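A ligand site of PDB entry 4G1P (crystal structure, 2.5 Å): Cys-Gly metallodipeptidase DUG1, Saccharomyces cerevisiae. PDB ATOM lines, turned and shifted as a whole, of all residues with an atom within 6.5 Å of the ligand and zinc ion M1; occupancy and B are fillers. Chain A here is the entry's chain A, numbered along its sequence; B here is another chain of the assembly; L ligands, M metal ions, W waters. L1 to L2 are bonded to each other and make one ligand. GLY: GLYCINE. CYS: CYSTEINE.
NH1 of Arg 348 is in hydrogen-bond range of O of CYS L2, 2.9 Å away. A nitrogen (N) of GLY L1 sits close to a ring nitrogen (NE2) of His 233 of chain B, 2.9 Å away. NE2 of His 385 lies close to SG of CYS L2, 3.1 Å away. SG of Cys 218 sits close to SG of CYS L2 (3.7 Å).
The side-chain carboxylate (OD1) of Asp 137 lies within hydrogen-bond range of a ring nitrogen (NE2) of His 102. OG1 of Thr 335 of chain B is in hydrogen-bond range of ND1 of His 450, at 3.3 Å. NH1 of Arg 348 is in hydrogen-bond range of OG of Ser 422 (2.7 Å). The side-chain hydroxyl of Ser 234 of chain B sits at hydrogen-bond distance from the guanidinium group of Arg 348 (3.3 Å). N of Gly 235 of chain B sits at hydrogen-bond distance from ND1 of His 233 of chain B. O of His 385 lies within hydrogen-bond range of N of Tyr 220 (2.8 Å). NE2 of His 102 is in hydrogen-bond range of OE1 of Glu 171 (3.3 Å). The backbone carbonyl oxygen (O) of Thr 335 of chain B is in hydrogen-bond range of the backbone NH (N) of Ser 234 of chain B.
An oxygen (O) of GLY L1 lies close to the side-chain carboxylate of Glu 171 (3.1 Å). O of Ser 422 sits close to O of GLY L1 (3.0 Å). OG1 of Thr 335 of chain B touches CA of CYS L2, 3.2 Å away.
Within 4 Å of zinc ion M1: Asp 137, Glu 172 and His 450.
OD2 of Asp 137 binds zinc ion M1. A ring nitrogen (NE2) of His 450 binds zinc ion M1. OE2 of Glu 172 binds zinc ion M1, at 2.1 Å. N of GLY L1 is bound to zinc ion M1, 2.6 Å away. Zinc ion M1 has four donor atoms within binding distance. Slightly farther from zinc ion M1 lies OE1 of Glu 172 (2.6 Å).
Water W1 bridges a sulfur (SG) of CYS L2 (3.0 Å) and the backbone carbonyl oxygen of Cys 218 (3.4 Å).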
ATOM      1  N   HIS A 102      16.021 -37.825 -24.496  1.00  0.00           N
ATOM      2  CA  HIS A 102      17.241 -37.033 -24.537  1.00  0.00           C
ATOM      3  C   HIS A 102      17.891 -36.882 -23.198  1.00  0.00           C
ATOM      4  O   HIS A 102      17.216 -36.676 -22.173  1.00  0.00           O
ATOM      5  CB  HIS A 102      17.008 -35.672 -25.208  1.00  0.00           C
ATOM      6  CG  HIS A 102      16.149 -34.730 -24.420  1.00  0.00           C
ATOM      7  ND1 HIS A 102      16.671 -33.863 -23.485  1.00  0.00           N
ATOM      8  CD2 HIS A 102      14.822 -34.465 -24.472  1.00  0.00           C
ATOM      9  CE1 HIS A 102      15.694 -33.134 -22.977  1.00  0.00           C
ATOM     10  NE2 HIS A 102      14.561 -33.476 -23.560  1.00  0.00           N
ATOM     11  N   GLN A 106      18.632 -28.486 -19.668  1.00  0.00           N
ATOM     12  CA  GLN A 106      18.737 -27.025 -19.546  1.00  0.00           C
ATOM     13  C   GLN A 106      19.765 -26.614 -18.479  1.00  0.00           C
ATOM     14  O   GLN A 106      19.998 -27.341 -17.533  1.00  0.00           O
ATOM     15  CB  GLN A 106      17.365 -26.441 -19.194  1.00  0.00           C
ATOM     16  CG  GLN A 106      16.376 -26.460 -20.340  1.00  0.00           C
ATOM     17  CD  GLN A 106      16.688 -25.414 -21.383  1.00  0.00           C
ATOM     18  OE1 GLN A 106      16.889 -24.248 -21.057  1.00  0.00           O
ATOM     19  NE2 GLN A 106      16.752 -25.829 -22.659  1.00  0.00           N
ATOM     20  N   ASP A 137      12.634 -33.590 -17.597  1.00  0.00           N
ATOM     21  CA  ASP A 137      12.948 -33.195 -18.958  1.00  0.00           C
ATOM     22  C   ASP A 137      14.450 -33.350 -19.152  1.00  0.00           C
ATOM     23  O   ASP A 137      15.178 -32.366 -18.997  1.00  0.00           O
ATOM     24  CB  ASP A 137      12.507 -31.733 -19.165  1.00  0.00           C
ATOM     25  CG  ASP A 137      12.811 -31.209 -20.558  1.00  0.00           C
ATOM     26  OD1 ASP A 137      13.139 -32.003 -21.462  1.00  0.00           O
ATOM     27  OD2 ASP A 137      12.694 -29.983 -20.773  1.00  0.00           O
ATOM     28  N   ASP A 138      14.915 -34.547 -19.503  1.00  0.00           N
ATOM     29  CA  ASP A 138      14.109 -35.693 -19.897  1.00  0.00           C
ATOM     30  C   ASP A 138      14.709 -36.971 -19.310  1.00  0.00           C
ATOM     31  O   ASP A 138      14.451 -38.064 -19.791  1.00  0.00           O
ATOM     32  CB  ASP A 138      14.099 -35.793 -21.437  1.00  0.00           C
ATOM     33  CG  ASP A 138      13.152 -36.874 -21.987  1.00  0.00           C
ATOM     34  OD1 ASP A 138      12.009 -37.014 -21.497  1.00  0.00           O
ATOM     35  OD2 ASP A 138      13.558 -37.592 -22.928  1.00  0.00           O
ATOM     36  N   GLU A 171      19.022 -32.164 -27.511  1.00  0.00           N
ATOM     37  CA  GLU A 171      17.623 -31.773 -27.628  1.00  0.00           C
ATOM     38  C   GLU A 171      17.385 -30.344 -27.158  1.00  0.00           C
ATOM     39  O   GLU A 171      16.595 -29.614 -27.749  1.00  0.00           O
ATOM     40  CB  GLU A 171      16.696 -32.730 -26.891  1.00  0.00           C
ATOM     41  CG  GLU A 171      15.257 -32.751 -27.390  1.00  0.00           C
ATOM     42  CD  GLU A 171      14.325 -31.820 -26.621  1.00  0.00           C
ATOM     43  OE1 GLU A 171      14.791 -31.063 -25.745  1.00  0.00           O
ATOM     44  OE2 GLU A 171      13.099 -31.842 -26.908  1.00  0.00           O
ATOM     45  N   GLU A 172      18.095 -29.935 -26.111  1.00  0.00           N
ATOM     46  CA  GLU A 172      17.931 -28.588 -25.570  1.00  0.00           C
ATOM     47  C   GLU A 172      18.744 -27.571 -26.382  1.00  0.00           C
ATOM     48  O   GLU A 172      18.800 -26.390 -26.029  1.00  0.00           O
ATOM     49  CB  GLU A 172      18.319 -28.548 -24.089  1.00  0.00           C
ATOM     50  CG  GLU A 172      17.596 -29.551 -23.194  1.00  0.00           C
ATOM     51  CD  GLU A 172      16.147 -29.168 -22.921  1.00  0.00           C
ATOM     52  OE1 GLU A 172      15.694 -28.115 -23.416  1.00  0.00           O
ATOM     53  OE2 GLU A 172      15.454 -29.924 -22.203  1.00  0.00           O
ATOM     54  N   SER A 173      19.355 -28.038 -27.459  1.00  0.00           N
ATOM     55  CA  SER A 173      20.219 -27.204 -28.293  1.00  0.00           C
ATOM     56  C   SER A 173      19.964 -27.456 -29.789  1.00  0.00           C
ATOM     57  O   SER A 173      20.901 -27.566 -30.582  1.00  0.00           O
ATOM     58  CB  SER A 173      21.688 -27.462 -27.946  1.00  0.00           C
ATOM     59  OG  SER A 173      21.934 -27.282 -26.562  1.00  0.00           O
ATOM     60  N   GLY A 174      18.689 -27.579 -30.147  1.00  0.00           N
ATOM     61  CA  GLY A 174      18.299 -27.716 -31.540  1.00  0.00           C
ATOM     62  C   GLY A 174      18.304 -29.107 -32.147  1.00  0.00           C
ATOM     63  O   GLY A 174      18.002 -29.249 -33.333  1.00  0.00           O
ATOM     64  N   ASP A 200       8.406 -37.488 -23.507  1.00  0.00           N
ATOM     65  CA  ASP A 200       9.157 -36.242 -23.436  1.00  0.00           C
ATOM     66  C   ASP A 200       8.226 -35.048 -23.335  1.00  0.00           C
ATOM     67  O   ASP A 200       8.507 -33.980 -23.888  1.00  0.00           O
ATOM     68  CB  ASP A 200      10.026 -36.105 -24.682  1.00  0.00           C
ATOM     69  CG  ASP A 200      11.293 -35.306 -24.432  1.00  0.00           C
ATOM     70  OD1 ASP A 200      11.487 -34.802 -23.306  1.00  0.00           O
ATOM     71  OD2 ASP A 200      12.101 -35.170 -25.364  1.00  0.00           O
ATOM     72  N   TYR A 202       4.350 -33.803 -20.822  1.00  0.00           N
ATOM     73  CA  TYR A 202       3.713 -33.823 -19.500  1.00  0.00           C
ATOM     74  C   TYR A 202       2.216 -33.902 -19.640  1.00  0.00           C
ATOM     75  O   TYR A 202       1.675 -33.595 -20.704  1.00  0.00           O
ATOM     76  CB  TYR A 202       4.068 -32.554 -18.723  1.00  0.00           C
ATOM     77  CG  TYR A 202       5.444 -32.075 -19.108  1.00  0.00           C
ATOM     78  CD1 TYR A 202       5.622 -31.203 -20.178  1.00  0.00           C
ATOM     79  CD2 TYR A 202       6.571 -32.562 -18.457  1.00  0.00           C
ATOM     80  CE1 TYR A 202       6.891 -30.811 -20.578  1.00  0.00           C
ATOM     81  CE2 TYR A 202       7.829 -32.166 -18.837  1.00  0.00           C
ATOM     82  CZ  TYR A 202       7.995 -31.290 -19.888  1.00  0.00           C
ATOM     83  OH  TYR A 202       9.269 -30.902 -20.279  1.00  0.00           O
ATOM     84  N   CYS A 218       8.678 -25.067 -33.414  1.00  0.00           N
ATOM     85  CA  CYS A 218       9.341 -23.927 -32.802  1.00  0.00           C
ATOM     86  C   CYS A 218      10.398 -23.327 -33.736  1.00  0.00           C
ATOM     87  O   CYS A 218      11.299 -24.022 -34.228  1.00  0.00           O
ATOM     88  CB  CYS A 218       9.951 -24.313 -31.448  1.00  0.00           C
ATOM     89  SG  CYS A 218      10.623 -22.897 -30.513  1.00  0.00           S
ATOM     90  N   ASN A 219      10.268 -22.038 -33.998  1.00  0.00           N
ATOM     91  CA  ASN A 219      11.275 -21.315 -34.770  1.00  0.00           C
ATOM     92  C   ASN A 219      11.942 -20.284 -33.863  1.00  0.00           C
ATOM     93  O   ASN A 219      11.270 -19.395 -33.317  1.00  0.00           O
ATOM     94  CB  ASN A 219      10.659 -20.658 -36.010  1.00  0.00           C
ATOM     95  CG  ASN A 219      10.439 -21.645 -37.140  1.00  0.00           C
ATOM     96  OD1 ASN A 219      10.276 -22.842 -36.914  1.00  0.00           O
ATOM     97  ND2 ASN A 219      10.437 -21.147 -38.367  1.00  0.00           N
ATOM     98  N   TYR A 220      13.236 -20.420 -33.667  1.00  0.00           N
ATOM     99  CA  TYR A 220      13.913 -19.544 -32.727  1.00  0.00           C
ATOM    100  C   TYR A 220      14.769 -18.529 -33.476  1.00  0.00           C
ATOM    101  O   TYR A 220      15.647 -18.911 -34.269  1.00  0.00           O
ATOM    102  CB  TYR A 220      14.769 -20.355 -31.752  1.00  0.00           C
ATOM    103  CG  TYR A 220      15.036 -19.653 -30.438  1.00  0.00           C
ATOM    104  CD1 TYR A 220      15.938 -18.610 -30.362  1.00  0.00           C
ATOM    105  CD2 TYR A 220      14.376 -20.036 -29.281  1.00  0.00           C
ATOM    106  CE1 TYR A 220      16.178 -17.955 -29.165  1.00  0.00           C
ATOM    107  CE2 TYR A 220      14.617 -19.406 -28.084  1.00  0.00           C
ATOM    108  CZ  TYR A 220      15.519 -18.359 -28.030  1.00  0.00           C
ATOM    109  OH  TYR A 220      15.786 -17.720 -26.841  1.00  0.00           O
ATOM    110  N   ARG A 348       6.003 -20.408 -31.775  1.00  0.00           N
ATOM    111  CA  ARG A 348       5.472 -21.757 -31.757  1.00  0.00           C
ATOM    112  C   ARG A 348       4.604 -21.968 -32.986  1.00  0.00           C
ATOM    113  O   ARG A 348       3.612 -21.284 -33.170  1.00  0.00           O
ATOM    114  CB  ARG A 348       4.677 -22.005 -30.476  1.00  0.00           C
ATOM    115  CG  ARG A 348       5.522 -21.954 -29.201  1.00  0.00           C
ATOM    116  CD  ARG A 348       6.464 -23.144 -29.079  1.00  0.00           C
ATOM    117  NE  ARG A 348       7.413 -22.936 -27.996  1.00  0.00           N
ATOM    118  CZ  ARG A 348       8.290 -23.850 -27.564  1.00  0.00           C
ATOM    119  NH1 ARG A 348       8.330 -25.075 -28.088  1.00  0.00           N
ATOM    120  NH2 ARG A 348       9.119 -23.530 -26.565  1.00  0.00           N
ATOM    121  N   HIS A 385      17.322 -21.931 -34.694  1.00  0.00           N
ATOM    122  CA  HIS A 385      16.910 -23.305 -34.980  1.00  0.00           C
ATOM    123  C   HIS A 385      15.423 -23.399 -35.286  1.00  0.00           C
ATOM    124  O   HIS A 385      14.631 -22.546 -34.867  1.00  0.00           O
ATOM    125  CB  HIS A 385      17.324 -24.267 -33.867  1.00  0.00           C
ATOM    126  CG  HIS A 385      16.550 -24.122 -32.597  1.00  0.00           C
ATOM    127  ND1 HIS A 385      17.157 -23.853 -31.387  1.00  0.00           N
ATOM    128  CD2 HIS A 385      15.224 -24.245 -32.324  1.00  0.00           C
ATOM    129  CE1 HIS A 385      16.238 -23.792 -30.434  1.00  0.00           C
ATOM    130  NE2 HIS A 385      15.055 -24.025 -30.980  1.00  0.00           N
ATOM    131  N   GLY A 420       1.653 -27.769 -26.162  1.00  0.00           N
ATOM    132  CA  GLY A 420       2.196 -26.452 -26.463  1.00  0.00           C
ATOM    133  C   GLY A 420       3.687 -26.540 -26.741  1.00  0.00           C
ATOM    134  O   GLY A 420       4.236 -25.766 -27.527  1.00  0.00           O
ATOM    135  N   GLY A 421       4.346 -27.495 -26.096  1.00  0.00           N
ATOM    136  CA  GLY A 421       5.774 -27.690 -26.273  1.00  0.00           C
ATOM    137  C   GLY A 421       6.100 -28.356 -27.595  1.00  0.00           C
ATOM    138  O   GLY A 421       5.197 -28.590 -28.401  1.00  0.00           O
ATOM    139  N   SER A 422       7.370 -28.688 -27.785  1.00  0.00           N
ATOM    140  CA  SER A 422       7.860 -29.216 -29.048  1.00  0.00           C
ATOM    141  C   SER A 422       8.827 -30.359 -28.869  1.00  0.00           C
ATOM    142  O   SER A 422       9.623 -30.377 -27.936  1.00  0.00           O
ATOM    143  CB  SER A 422       8.566 -28.118 -29.809  1.00  0.00           C
ATOM    144  OG  SER A 422       7.726 -27.005 -29.917  1.00  0.00           O
ATOM    145  N   ILE A 423       8.758 -31.325 -29.761  1.00  0.00           N
ATOM    146  CA  ILE A 423       9.773 -32.352 -29.825  1.00  0.00           C
ATOM    147  C   ILE A 423      10.154 -32.495 -31.282  1.00  0.00           C
ATOM    148  O   ILE A 423       9.650 -33.340 -31.977  1.00  0.00           O
ATOM    149  CB  ILE A 423       9.284 -33.691 -29.298  1.00  0.00           C
ATOM    150  CG1 ILE A 423       8.689 -33.524 -27.899  1.00  0.00           C
ATOM    151  CG2 ILE A 423      10.416 -34.683 -29.294  1.00  0.00           C
ATOM    152  CD1 ILE A 423       7.903 -34.733 -27.402  1.00  0.00           C
ATOM    153  N   PRO A 424      11.047 -31.621 -31.741  1.00  0.00           N
ATOM    154  CA  PRO A 424      11.473 -31.492 -33.143  1.00  0.00           C
ATOM    155  C   PRO A 424      11.513 -32.767 -34.011  1.00  0.00           C
ATOM    156  O   PRO A 424      10.965 -32.677 -35.097  1.00  0.00           O
ATOM    157  CB  PRO A 424      12.855 -30.866 -33.000  1.00  0.00           C
ATOM    158  CG  PRO A 424      12.683 -29.950 -31.829  1.00  0.00           C
ATOM    159  CD  PRO A 424      11.746 -30.650 -30.877  1.00  0.00           C
ATOM    160  N   ALA A 449       9.684 -27.760 -15.885  1.00  0.00           N
ATOM    161  CA  ALA A 449      10.709 -27.899 -16.911  1.00  0.00           C
ATOM    162  C   ALA A 449      11.159 -26.516 -17.413  1.00  0.00           C
ATOM    163  O   ALA A 449      10.336 -25.608 -17.574  1.00  0.00           O
ATOM    164  CB  ALA A 449      10.215 -28.747 -18.066  1.00  0.00           C
ATOM    165  N   HIS A 450      12.469 -26.372 -17.609  1.00  0.00           N
ATOM    166  CA  HIS A 450      13.088 -25.125 -18.072  1.00  0.00           C
ATOM    167  C   HIS A 450      12.990 -24.020 -17.028  1.00  0.00           C
ATOM    168  O   HIS A 450      13.165 -22.842 -17.339  1.00  0.00           O
ATOM    169  CB  HIS A 450      12.478 -24.648 -19.396  1.00  0.00           C
ATOM    170  CG  HIS A 450      12.714 -25.585 -20.536  1.00  0.00           C
ATOM    171  ND1 HIS A 450      12.631 -25.177 -21.850  1.00  0.00           N
ATOM    172  CD2 HIS A 450      13.022 -26.901 -20.570  1.00  0.00           C
ATOM    173  CE1 HIS A 450      12.887 -26.206 -22.647  1.00  0.00           C
ATOM    174  NE2 HIS A 450      13.125 -27.262 -21.888  1.00  0.00           N
ATOM    175  N   HIS B 233       8.232 -22.424 -19.069  1.00  0.00           N
ATOM    176  CA  HIS B 233       8.575 -23.036 -20.350  1.00  0.00           C
ATOM    177  C   HIS B 233       7.782 -22.285 -21.418  1.00  0.00           C
ATOM    178  O   HIS B 233       6.565 -22.194 -21.337  1.00  0.00           O
ATOM    179  CB  HIS B 233       8.193 -24.514 -20.328  1.00  0.00           C
ATOM    180  CG  HIS B 233       8.605 -25.274 -21.552  1.00  0.00           C
ATOM    181  ND1 HIS B 233       8.060 -25.018 -22.792  1.00  0.00           N
ATOM    182  CD2 HIS B 233       9.511 -26.262 -21.727  1.00  0.00           C
ATOM    183  CE1 HIS B 233       8.612 -25.836 -23.679  1.00  0.00           C
ATOM    184  NE2 HIS B 233       9.497 -26.595 -23.062  1.00  0.00           N
ATOM    185  N   SER B 234       8.471 -21.722 -22.400  1.00  0.00           N
ATOM    186  CA  SER B 234       7.768 -20.817 -23.298  1.00  0.00           C
ATOM    187  C   SER B 234       6.835 -21.541 -24.263  1.00  0.00           C
ATOM    188  O   SER B 234       6.065 -20.889 -24.958  1.00  0.00           O
ATOM    189  CB  SER B 234       8.729 -19.888 -24.061  1.00  0.00           C
ATOM    190  OG  SER B 234       9.337 -20.568 -25.138  1.00  0.00           O
ATOM    191  N   GLY B 235       6.922 -22.878 -24.276  1.00  0.00           N
ATOM    192  CA  GLY B 235       6.098 -23.698 -25.146  1.00  0.00           C
ATOM    193  C   GLY B 235       4.830 -24.151 -24.453  1.00  0.00           C
ATOM    194  O   GLY B 235       3.745 -24.098 -25.010  1.00  0.00           O
ATOM    195  N   THR B 335      14.284 -21.293 -24.494  1.00  0.00           N
ATOM    196  CA  THR B 335      12.839 -21.186 -24.658  1.00  0.00           C
ATOM    197  C   THR B 335      12.224 -21.013 -23.294  1.00  0.00           C
ATOM    198  O   THR B 335      11.723 -21.975 -22.699  1.00  0.00           O
ATOM    199  CB  THR B 335      12.252 -22.430 -25.293  1.00  0.00           C
ATOM    200  OG1 THR B 335      12.898 -23.584 -24.768  1.00  0.00           O
ATOM    201  CG2 THR B 335      12.439 -22.410 -26.788  1.00  0.00           C
HETATM  202  N   GLY L   1      11.291 -28.825 -23.685  1.00  0.00           N
HETATM  203  CA  GLY L   1      12.388 -29.330 -24.492  1.00  0.00           C
HETATM  204  C   GLY L   1      12.375 -28.488 -25.738  1.00  0.00           C
HETATM  205  O   GLY L   1      11.967 -28.940 -26.813  1.00  0.00           O
HETATM  206  N   CYS L   2      12.816 -27.242 -25.582  1.00  0.00           N
HETATM  207  CA  CYS L   2      12.601 -26.209 -26.576  1.00  0.00           C
HETATM  208  C   CYS L   2      11.106 -25.874 -26.638  1.00  0.00           C
HETATM  209  O   CYS L   2      10.267 -26.749 -26.823  1.00  0.00           O
HETATM  210  CB  CYS L   2      13.145 -26.647 -27.943  1.00  0.00           C
HETATM  211  SG  CYS L   2      12.977 -25.432 -29.211  1.00  0.00           S
HETATM  212 ZN    ZN M   1      13.530 -29.176 -22.427  1.00  0.00          ZN
HETATM  213 ZN    ZN M   2      11.023 -32.108 -23.387  1.00  0.00          ZN
HETATM  214  O   HOH W   1      12.323 -26.367 -31.998  1.00  0.00           O
HETATM  215  O   HOH W   2      16.493 -26.950 -28.524  1.00  0.00           O
